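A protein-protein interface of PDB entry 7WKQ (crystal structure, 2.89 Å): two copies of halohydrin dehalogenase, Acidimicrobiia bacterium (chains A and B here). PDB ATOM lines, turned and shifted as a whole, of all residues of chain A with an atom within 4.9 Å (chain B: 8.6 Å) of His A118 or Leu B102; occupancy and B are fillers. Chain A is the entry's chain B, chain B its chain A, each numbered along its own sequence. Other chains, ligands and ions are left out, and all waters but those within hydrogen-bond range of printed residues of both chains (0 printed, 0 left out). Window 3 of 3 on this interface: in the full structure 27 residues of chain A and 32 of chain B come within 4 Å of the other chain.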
ATOM      1  N   LEU A  62     -13.160  -1.313  -7.104  1.00  0.00           N
ATOM      2  CA  LEU A  62     -13.639   0.082  -7.233  1.00  0.00           C
ATOM      3  C   LEU A  62     -13.940   0.383  -8.696  1.00  0.00           C
ATOM      4  O   LEU A  62     -14.574   1.409  -8.954  1.00  0.00           O
ATOM      5  CB  LEU A  62     -12.599   1.024  -6.626  1.00  0.00           C
ATOM      6  CG  LEU A  62     -12.508   0.997  -5.106  1.00  0.00           C
ATOM      7  CD1 LEU A  62     -11.357   1.862  -4.632  1.00  0.00           C
ATOM      8  CD2 LEU A  62     -13.814   1.462  -4.487  1.00  0.00           C
ATOM      9  N   ALA A  63     -13.494  -0.474  -9.611  1.00  0.00           N
ATOM     10  CA  ALA A  63     -13.844  -0.310 -11.036  1.00  0.00           C
ATOM     11  C   ALA A  63     -15.353  -0.443 -11.149  1.00  0.00           C
ATOM     12  O   ALA A  63     -15.917   0.196 -12.026  1.00  0.00           O
ATOM     13  CB  ALA A  63     -13.151  -1.344 -11.863  1.00  0.00           C
ATOM     14  N   ASP A  64     -15.944  -1.311 -10.335  1.00  0.00           N
ATOM     15  CA  ASP A  64     -17.418  -1.430 -10.310  1.00  0.00           C
ATOM     16  C   ASP A  64     -17.969  -0.049  -9.971  1.00  0.00           C
ATOM     17  O   ASP A  64     -17.803   0.358  -8.817  1.00  0.00           O
ATOM     18  CB  ASP A  64     -17.905  -2.470  -9.302  1.00  0.00           C
ATOM     19  CG  ASP A  64     -19.392  -2.758  -9.363  1.00  0.00           C
ATOM     20  OD1 ASP A  64     -20.060  -2.227 -10.266  1.00  0.00           O
ATOM     21  OD2 ASP A  64     -19.867  -3.520  -8.506  1.00  0.00           O
ATOM     22  N   PRO A  65     -18.612   0.696 -10.895  1.00  0.00           N
ATOM     23  CA  PRO A  65     -19.196   1.993 -10.520  1.00  0.00           C
ATOM     24  C   PRO A  65     -19.977   1.895  -9.225  1.00  0.00           C
ATOM     25  O   PRO A  65     -19.920   2.804  -8.380  1.00  0.00           O
ATOM     26  CB  PRO A  65     -20.087   2.330 -11.723  1.00  0.00           C
ATOM     27  CG  PRO A  65     -19.435   1.652 -12.871  1.00  0.00           C
ATOM     28  CD  PRO A  65     -18.846   0.368 -12.310  1.00  0.00           C
ATOM     29  N   ALA A  68     -17.832   2.023  -5.032  1.00  0.00           N
ATOM     30  CA  ALA A  68     -17.564   3.284  -4.328  1.00  0.00           C
ATOM     31  C   ALA A  68     -18.863   3.968  -3.928  1.00  0.00           C
ATOM     32  O   ALA A  68     -18.975   4.518  -2.825  1.00  0.00           O
ATOM     33  CB  ALA A  68     -16.714   4.213  -5.192  1.00  0.00           C
ATOM     34  N   GLU A 114      -9.721   3.679 -13.882  1.00  0.00           N
ATOM     35  CA  GLU A 114     -11.152   3.656 -13.613  1.00  0.00           C
ATOM     36  C   GLU A 114     -11.442   3.561 -12.117  1.00  0.00           C
ATOM     37  O   GLU A 114     -12.351   4.241 -11.616  1.00  0.00           O
ATOM     38  CB  GLU A 114     -11.812   2.526 -14.396  1.00  0.00           C
ATOM     39  CG  GLU A 114     -11.544   2.610 -15.895  1.00  0.00           C
ATOM     40  CD  GLU A 114     -12.454   1.719 -16.725  1.00  0.00           C
ATOM     41  OE1 GLU A 114     -12.254   1.672 -17.966  1.00  0.00           O
ATOM     42  OE2 GLU A 114     -13.375   1.089 -16.143  1.00  0.00           O
ATOM     43  N   ALA A 115     -10.688   2.710 -11.382  1.00  0.00           N
ATOM     44  CA  ALA A 115     -10.930   2.560  -9.944  1.00  0.00           C
ATOM     45  C   ALA A 115     -10.743   3.872  -9.194  1.00  0.00           C
ATOM     46  O   ALA A 115     -11.656   4.259  -8.433  1.00  0.00           O
ATOM     47  CB  ALA A 115     -10.051   1.440  -9.380  1.00  0.00           C
ATOM     48  N   PRO A 116      -9.652   4.636  -9.391  1.00  0.00           N
ATOM     49  CA  PRO A 116      -9.606   5.964  -8.749  1.00  0.00           C
ATOM     50  C   PRO A 116     -10.694   6.895  -9.252  1.00  0.00           C
ATOM     51  O   PRO A 116     -11.423   7.453  -8.427  1.00  0.00           O
ATOM     52  CB  PRO A 116      -8.218   6.506  -9.110  1.00  0.00           C
ATOM     53  CG  PRO A 116      -7.641   5.597 -10.073  1.00  0.00           C
ATOM     54  CD  PRO A 116      -8.423   4.323 -10.131  1.00  0.00           C
ATOM     55  N   TYR A 117     -10.919   6.956 -10.568  1.00  0.00           N
ATOM     56  CA  TYR A 117     -11.961   7.823 -11.111  1.00  0.00           C
ATOM     57  C   TYR A 117     -13.280   7.648 -10.359  1.00  0.00           C
ATOM     58  O   TYR A 117     -13.849   8.618  -9.828  1.00  0.00           O
ATOM     59  CB  TYR A 117     -12.127   7.573 -12.615  1.00  0.00           C
ATOM     60  CG  TYR A 117     -13.243   8.379 -13.255  1.00  0.00           C
ATOM     61  CD1 TYR A 117     -13.057   9.707 -13.618  1.00  0.00           C
ATOM     62  CD2 TYR A 117     -14.490   7.817 -13.488  1.00  0.00           C
ATOM     63  CE1 TYR A 117     -14.087  10.446 -14.202  1.00  0.00           C
ATOM     64  CE2 TYR A 117     -15.517   8.544 -14.066  1.00  0.00           C
ATOM     65  CZ  TYR A 117     -15.310   9.851 -14.425  1.00  0.00           C
ATOM     66  OH  TYR A 117     -16.340  10.565 -15.006  1.00  0.00           O
ATOM     67  N   HIS A 118     -13.788   6.412 -10.333  1.00  0.00           N
ATOM     68  CA  HIS A 118     -15.045   6.135  -9.640  1.00  0.00           C
ATOM     69  C   HIS A 118     -14.961   6.500  -8.161  1.00  0.00           C
ATOM     70  O   HIS A 118     -15.895   7.124  -7.610  1.00  0.00           O
ATOM     71  CB  HIS A 118     -15.421   4.669  -9.820  1.00  0.00           C
ATOM     72  CG  HIS A 118     -16.022   4.389 -11.156  1.00  0.00           C
ATOM     73  ND1 HIS A 118     -15.475   3.485 -12.042  1.00  0.00           N
ATOM     74  CD2 HIS A 118     -17.098   4.926 -11.779  1.00  0.00           C
ATOM     75  CE1 HIS A 118     -16.198   3.460 -13.148  1.00  0.00           C
ATOM     76  NE2 HIS A 118     -17.190   4.324 -13.013  1.00  0.00           N
ATOM     77  N   PHE A 119     -13.829   6.234  -7.524  1.00  0.00           N
ATOM     78  CA  PHE A 119     -13.671   6.619  -6.099  1.00  0.00           C
ATOM     79  C   PHE A 119     -13.854   8.121  -5.945  1.00  0.00           C
ATOM     80  O   PHE A 119     -14.704   8.544  -5.167  1.00  0.00           O
ATOM     81  CB  PHE A 119     -12.290   6.230  -5.579  1.00  0.00           C
ATOM     82  CG  PHE A 119     -12.042   6.482  -4.115  1.00  0.00           C
ATOM     83  CD1 PHE A 119     -12.823   5.874  -3.149  1.00  0.00           C
ATOM     84  CD2 PHE A 119     -11.009   7.307  -3.707  1.00  0.00           C
ATOM     85  CE1 PHE A 119     -12.585   6.100  -1.804  1.00  0.00           C
ATOM     86  CE2 PHE A 119     -10.775   7.535  -2.363  1.00  0.00           C
ATOM     87  CZ  PHE A 119     -11.562   6.930  -1.416  1.00  0.00           C
ATOM     88  N   LEU A 120     -13.073   8.903  -6.676  1.00  0.00           N
ATOM     89  CA  LEU A 120     -13.116  10.371  -6.507  1.00  0.00           C
ATOM     90  C   LEU A 120     -14.495  10.891  -6.881  1.00  0.00           C
ATOM     91  O   LEU A 120     -15.011  11.741  -6.161  1.00  0.00           O
ATOM     92  CB  LEU A 120     -12.042  10.986  -7.405  1.00  0.00           C
ATOM     93  CG  LEU A 120     -10.610  10.547  -7.121  1.00  0.00           C
ATOM     94  CD1 LEU A 120      -9.650  11.195  -8.100  1.00  0.00           C
ATOM     95  CD2 LEU A 120     -10.221  10.893  -5.698  1.00  0.00           C
ATOM     96  N   LYS A 121     -15.094  10.344  -7.926  1.00  0.00           N
ATOM     97  CA  LYS A 121     -16.379  10.880  -8.437  1.00  0.00           C
ATOM     98  C   LYS A 121     -17.494  10.632  -7.423  1.00  0.00           C
ATOM     99  O   LYS A 121     -18.558  11.240  -7.545  1.00  0.00           O
ATOM    100  CB  LYS A 121     -16.586  10.413  -9.882  1.00  0.00           C
ATOM    101  CG  LYS A 121     -17.822  10.923 -10.600  1.00  0.00           C
ATOM    102  CD  LYS A 121     -17.876  10.428 -12.021  1.00  0.00           C
ATOM    103  CE  LYS A 121     -19.113  10.907 -12.745  1.00  0.00           C
ATOM    104  NZ  LYS A 121     -19.138  10.406 -14.136  1.00  0.00           N
ATOM    105  N   ALA A 122     -17.242   9.761  -6.458  1.00  0.00           N
ATOM    106  CA  ALA A 122     -18.264   9.439  -5.448  1.00  0.00           C
ATOM    107  C   ALA A 122     -17.955  10.146  -4.133  1.00  0.00           C
ATOM    108  O   ALA A 122     -18.895  10.647  -3.514  1.00  0.00           O
ATOM    109  CB  ALA A 122     -18.292   7.960  -5.245  1.00  0.00           C
ATOM    110  N   PHE B  97     -14.012  17.782 -13.614  1.00  0.00           N
ATOM    111  CA  PHE B  97     -14.029  16.355 -13.231  1.00  0.00           C
ATOM    112  C   PHE B  97     -15.368  16.003 -12.619  1.00  0.00           C
ATOM    113  O   PHE B  97     -15.934  14.970 -12.959  1.00  0.00           O
ATOM    114  CB  PHE B  97     -12.930  16.084 -12.210  1.00  0.00           C
ATOM    115  CG  PHE B  97     -12.802  14.660 -11.748  1.00  0.00           C
ATOM    116  CD1 PHE B  97     -12.078  13.742 -12.485  1.00  0.00           C
ATOM    117  CD2 PHE B  97     -13.381  14.248 -10.561  1.00  0.00           C
ATOM    118  CE1 PHE B  97     -11.942  12.437 -12.046  1.00  0.00           C
ATOM    119  CE2 PHE B  97     -13.253  12.940 -10.130  1.00  0.00           C
ATOM    120  CZ  PHE B  97     -12.534  12.037 -10.874  1.00  0.00           C
ATOM    121  N   ASP B  99     -18.191  16.906 -13.209  1.00  0.00           N
ATOM    122  CA  ASP B  99     -19.309  16.862 -14.183  1.00  0.00           C
ATOM    123  C   ASP B  99     -19.002  15.851 -15.283  1.00  0.00           C
ATOM    124  O   ASP B  99     -19.707  15.860 -16.294  1.00  0.00           O
ATOM    125  CB  ASP B  99     -19.544  18.252 -14.764  1.00  0.00           C
ATOM    126  CG  ASP B  99     -20.064  19.260 -13.757  1.00  0.00           C
ATOM    127  OD1 ASP B  99     -19.696  20.442 -13.876  1.00  0.00           O
ATOM    128  OD2 ASP B  99     -20.833  18.855 -12.868  1.00  0.00           O
ATOM    129  N   SER B 100     -17.993  15.010 -15.088  1.00  0.00           N
ATOM    130  CA  SER B 100     -17.547  14.091 -16.163  1.00  0.00           C
ATOM    131  C   SER B 100     -18.317  12.776 -16.177  1.00  0.00           C
ATOM    132  O   SER B 100     -19.233  12.654 -15.370  1.00  0.00           O
ATOM    133  CB  SER B 100     -16.079  13.846 -16.017  1.00  0.00           C
ATOM    134  OG  SER B 100     -15.794  13.186 -14.800  1.00  0.00           O
ATOM    135  N   THR B 101     -17.964  11.855 -17.083  1.00  0.00           N
ATOM    136  CA  THR B 101     -18.583  10.513 -17.206  1.00  0.00           C
ATOM    137  C   THR B 101     -17.495   9.514 -17.583  1.00  0.00           C
ATOM    138  O   THR B 101     -16.530   9.923 -18.225  1.00  0.00           O
ATOM    139  CB  THR B 101     -19.691  10.507 -18.259  1.00  0.00           C
ATOM    140  OG1 THR B 101     -19.273  11.314 -19.357  1.00  0.00           O
ATOM    141  CG2 THR B 101     -21.013  11.020 -17.733  1.00  0.00           C
ATOM    142  N   LEU B 102     -17.652   8.257 -17.185  1.00  0.00           N
ATOM    143  CA  LEU B 102     -16.683   7.209 -17.575  1.00  0.00           C
ATOM    144  C   LEU B 102     -16.621   7.188 -19.094  1.00  0.00           C
ATOM    145  O   LEU B 102     -15.589   6.802 -19.636  1.00  0.00           O
ATOM    146  CB  LEU B 102     -17.151   5.863 -17.026  1.00  0.00           C
ATOM    147  CG  LEU B 102     -16.120   4.740 -17.038  1.00  0.00           C
ATOM    148  CD1 LEU B 102     -14.973   5.056 -16.097  1.00  0.00           C
ATOM    149  CD2 LEU B 102     -16.767   3.422 -16.656  1.00  0.00           C
ATOM    150  N   GLU B 103     -17.703   7.604 -19.738  1.00  0.00           N
ATOM    151  CA  GLU B 103     -17.729   7.599 -21.220  1.00  0.00           C
ATOM    152  C   GLU B 103     -16.638   8.533 -21.717  1.00  0.00           C
ATOM    153  O   GLU B 103     -15.893   8.149 -22.624  1.00  0.00           O
ATOM    154  CB  GLU B 103     -19.111   8.045 -21.690  1.00  0.00           C
ATOM    155  CG  GLU B 103     -20.201   7.017 -21.441  1.00  0.00           C
ATOM    156  CD  GLU B 103     -20.685   6.902 -20.006  1.00  0.00           C
ATOM    157  OE1 GLU B 103     -20.330   5.915 -19.342  1.00  0.00           O
ATOM    158  OE2 GLU B 103     -21.418   7.798 -19.561  1.00  0.00           O
ATOM    159  N   ASP B 104     -16.537   9.701 -21.110  1.00  0.00           N
ATOM    160  CA  ASP B 104     -15.462  10.661 -21.440  1.00  0.00           C
ATOM    161  C   ASP B 104     -14.114  10.032 -21.083  1.00  0.00           C
ATOM    162  O   ASP B 104     -13.157  10.143 -21.906  1.00  0.00           O
ATOM    163  CB  ASP B 104     -15.707  11.958 -20.674  1.00  0.00           C
ATOM    164  CG  ASP B 104     -17.020  12.642 -21.006  1.00  0.00           C
ATOM    165  OD1 ASP B 104     -17.588  12.334 -22.065  1.00  0.00           O
ATOM    166  OD2 ASP B 104     -17.459  13.477 -20.199  1.00  0.00           O
ATOM    167  N   LEU B 105     -13.971   9.314 -19.975  1.00  0.00           N
ATOM    168  CA  LEU B 105     -12.625   8.748 -19.687  1.00  0.00           C
ATOM    169  C   LEU B 105     -12.280   7.714 -20.750  1.00  0.00           C
ATOM    170  O   LEU B 105     -11.119   7.613 -21.135  1.00  0.00           O
ATOM    171  CB  LEU B 105     -12.606   8.117 -18.295  1.00  0.00           C
ATOM    172  CG  LEU B 105     -11.323   7.386 -17.904  1.00  0.00           C
ATOM    173  CD1 LEU B 105     -10.148   8.344 -17.827  1.00  0.00           C
ATOM    174  CD2 LEU B 105     -11.497   6.665 -16.579  1.00  0.00           C
ATOM    175  N   HIS B 106     -13.269   6.958 -21.188  1.00  0.00           N
ATOM    176  CA  HIS B 106     -13.038   5.946 -22.237  1.00  0.00           C
ATOM    177  C   HIS B 106     -12.619   6.637 -23.520  1.00  0.00           C
ATOM    178  O   HIS B 106     -11.716   6.138 -24.177  1.00  0.00           O
ATOM    179  CB  HIS B 106     -14.331   5.190 -22.502  1.00  0.00           C
ATOM    180  CG  HIS B 106     -14.717   4.209 -21.452  1.00  0.00           C
ATOM    181  ND1 HIS B 106     -16.021   3.818 -21.247  1.00  0.00           N
ATOM    182  CD2 HIS B 106     -13.976   3.563 -20.529  1.00  0.00           C
ATOM    183  CE1 HIS B 106     -16.064   2.960 -20.251  1.00  0.00           C
ATOM    184  NE2 HIS B 106     -14.825   2.788 -19.794  1.00  0.00           N
ATOM    185  N   SER B 107     -13.254   7.752 -23.853  1.00  0.00           N
ATOM    186  CA  SER B 107     -12.970   8.399 -25.153  1.00  0.00           C
ATOM    187  C   SER B 107     -11.518   8.827 -25.189  1.00  0.00           C
ATOM    188  O   SER B 107     -10.848   8.577 -26.193  1.00  0.00           O
ATOM    189  CB  SER B 107     -13.852   9.570 -25.345  1.00  0.00           C
ATOM    190  OG  SER B 107     -14.145   9.754 -26.716  1.00  0.00           O
ATOM    191  N   VAL B 108     -11.061   9.433 -24.107  1.00  0.00           N
ATOM    192  CA  VAL B 108      -9.663   9.916 -24.066  1.00  0.00           C
ATOM    193  C   VAL B 108      -8.707   8.727 -24.088  1.00  0.00           C
ATOM    194  O   VAL B 108      -7.743   8.777 -24.843  1.00  0.00           O
ATOM    195  CB  VAL B 108      -9.439  10.880 -22.889  1.00  0.00           C
ATOM    196  CG1 VAL B 108     -10.258  12.146 -23.051  1.00  0.00           C
ATOM    197  CG2 VAL B 108      -9.687  10.260 -21.529  1.00  0.00           C
ATOM    198  N   VAL B 109      -8.989   7.685 -23.320  1.00  0.00           N
ATOM    199  CA  VAL B 109      -8.047   6.538 -23.238  1.00  0.00           C
ATOM    200  C   VAL B 109      -7.960   5.869 -24.604  1.00  0.00           C
ATOM    201  O   VAL B 109      -6.861   5.532 -25.034  1.00  0.00           O
ATOM    202  CB  VAL B 109      -8.455   5.551 -22.134  1.00  0.00           C
ATOM    203  CG1 VAL B 109      -7.828   4.182 -22.329  1.00  0.00           C
ATOM    204  CG2 VAL B 109      -8.129   6.095 -20.755  1.00  0.00           C
ATOM    205  N   GLN B 110      -9.090   5.696 -25.269  1.00  0.00           N
ATOM    206  CA  GLN B 110      -9.029   4.976 -26.549  1.00  0.00           C
ATOM    207  C   GLN B 110      -8.196   5.782 -27.527  1.00  0.00           C
ATOM    208  O   GLN B 110      -7.340   5.196 -28.180  1.00  0.00           O
ATOM    209  CB  GLN B 110     -10.438   4.833 -27.101  1.00  0.00           C
ATOM    210  CG  GLN B 110     -11.291   3.828 -26.345  1.00  0.00           C
ATOM    211  CD  GLN B 110     -12.742   3.901 -26.744  1.00  0.00           C
ATOM    212  OE1 GLN B 110     -13.099   4.506 -27.752  1.00  0.00           O
ATOM    213  NE2 GLN B 110     -13.596   3.280 -25.948  1.00  0.00           N
ATOM    214  N   LEU B 152      -9.238  14.642 -17.241  1.00  0.00           N
ATOM    215  CA  LEU B 152      -9.162  13.278 -17.754  1.00  0.00           C
ATOM    216  C   LEU B 152      -8.247  13.202 -18.961  1.00  0.00           C
ATOM    217  O   LEU B 152      -7.339  12.358 -19.008  1.00  0.00           O
ATOM    218  CB  LEU B 152     -10.560  12.799 -18.138  1.00  0.00           C
ATOM    219  CG  LEU B 152     -11.588  12.692 -17.016  1.00  0.00           C
ATOM    220  CD1 LEU B 152     -12.845  12.083 -17.590  1.00  0.00           C
ATOM    221  CD2 LEU B 152     -11.050  11.906 -15.801  1.00  0.00           C
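OG of Ser B100 is in hydrogen-bond range of OH of Tyr A117 (2.7 Å). The side-chain amino group (NZ) of Lys A121 is in hydrogen-bond range of the backbone carbonyl oxygen (O) of Ser B100, 2.6 Å away. N of Thr B101 is in hydrogen-bond range of OH of Tyr A117, 2.9 Å away. The backbone NH (N) of Leu B102 lies within hydrogen-bond range of the side-chain hydroxyl (OH) of Tyr A117 (3.4 Å). A ring nitrogen (NE2) of His B106 lies within hydrogen-bond range of the side-chain carboxylate (OE1) of Glu A114, 3.3 Å away. The backbone NH (N) of Thr B101 lies close to the side-chain amino group (NZ) of Lys A121 (3.5 Å).
Among the printed residues, merely in contact across the chains: Tyr A117 with Phe B97, His A118 with Leu B102, Leu A120 with Phe B97, Tyr A117 with Leu B152 and Lys A121 with Phe B97.
O of Phe B97 sits at hydrogen-bond distance from OG of Ser B100 (2.6 Å). The side-chain hydroxyl of Thr B101 sits at hydrogen-bond distance from the side-chain carboxylate of Asp B104 (2.9 Å). The backbone carbonyl oxygen of Leu B102 sits close to a ring nitrogen (ND1) of His B106 (3.4 Å). The backbone carbonyl oxygen (O) of Ala A63 is in hydrogen-bond range of a ring nitrogen (ND1) of His A118 (3.3 Å). The backbone carbonyl oxygen (O) of Glu A114 is in hydrogen-bond range of a ring nitrogen (ND1) of His A118. The side-chain hydroxyl (OH) of Tyr A117 lies within hydrogen-bond range of the side-chain amino group (NZ) of Lys A121 (2.9 Å).
Of the 14 printed residues of chain B, 6 touch a printed residue of chain A. Hydrophobic or aromatic side chains of chain A within 4 Å of the printed part of chain B: Tyr A117, His A118 and Leu A120. Along chain A the printed residues that touch a printed residue of chain B span positions 114 to 121. Among the printed residues, no Asp or Glu carboxylate lies within 4 Å of a Lys or Arg side-chain nitrogen of the other chain.
His A118 touches one residue of chain B. Of the printed residues of chain A, Leu B102 touches Tyr A117 and His A118. Of the printed residues of chain A, Thr B101 touches Tyr A117 and Lys A121. Printed residues of chain B within 4 Å of Glu A114: His B106. The nearest residue of chain B that does not touch His A118 is Phe B97 (5.8 Å). The nearest printed residue of chain B that does not touch Tyr A117 is Leu B105 (4.1 Å).
No position is printed for both chains.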
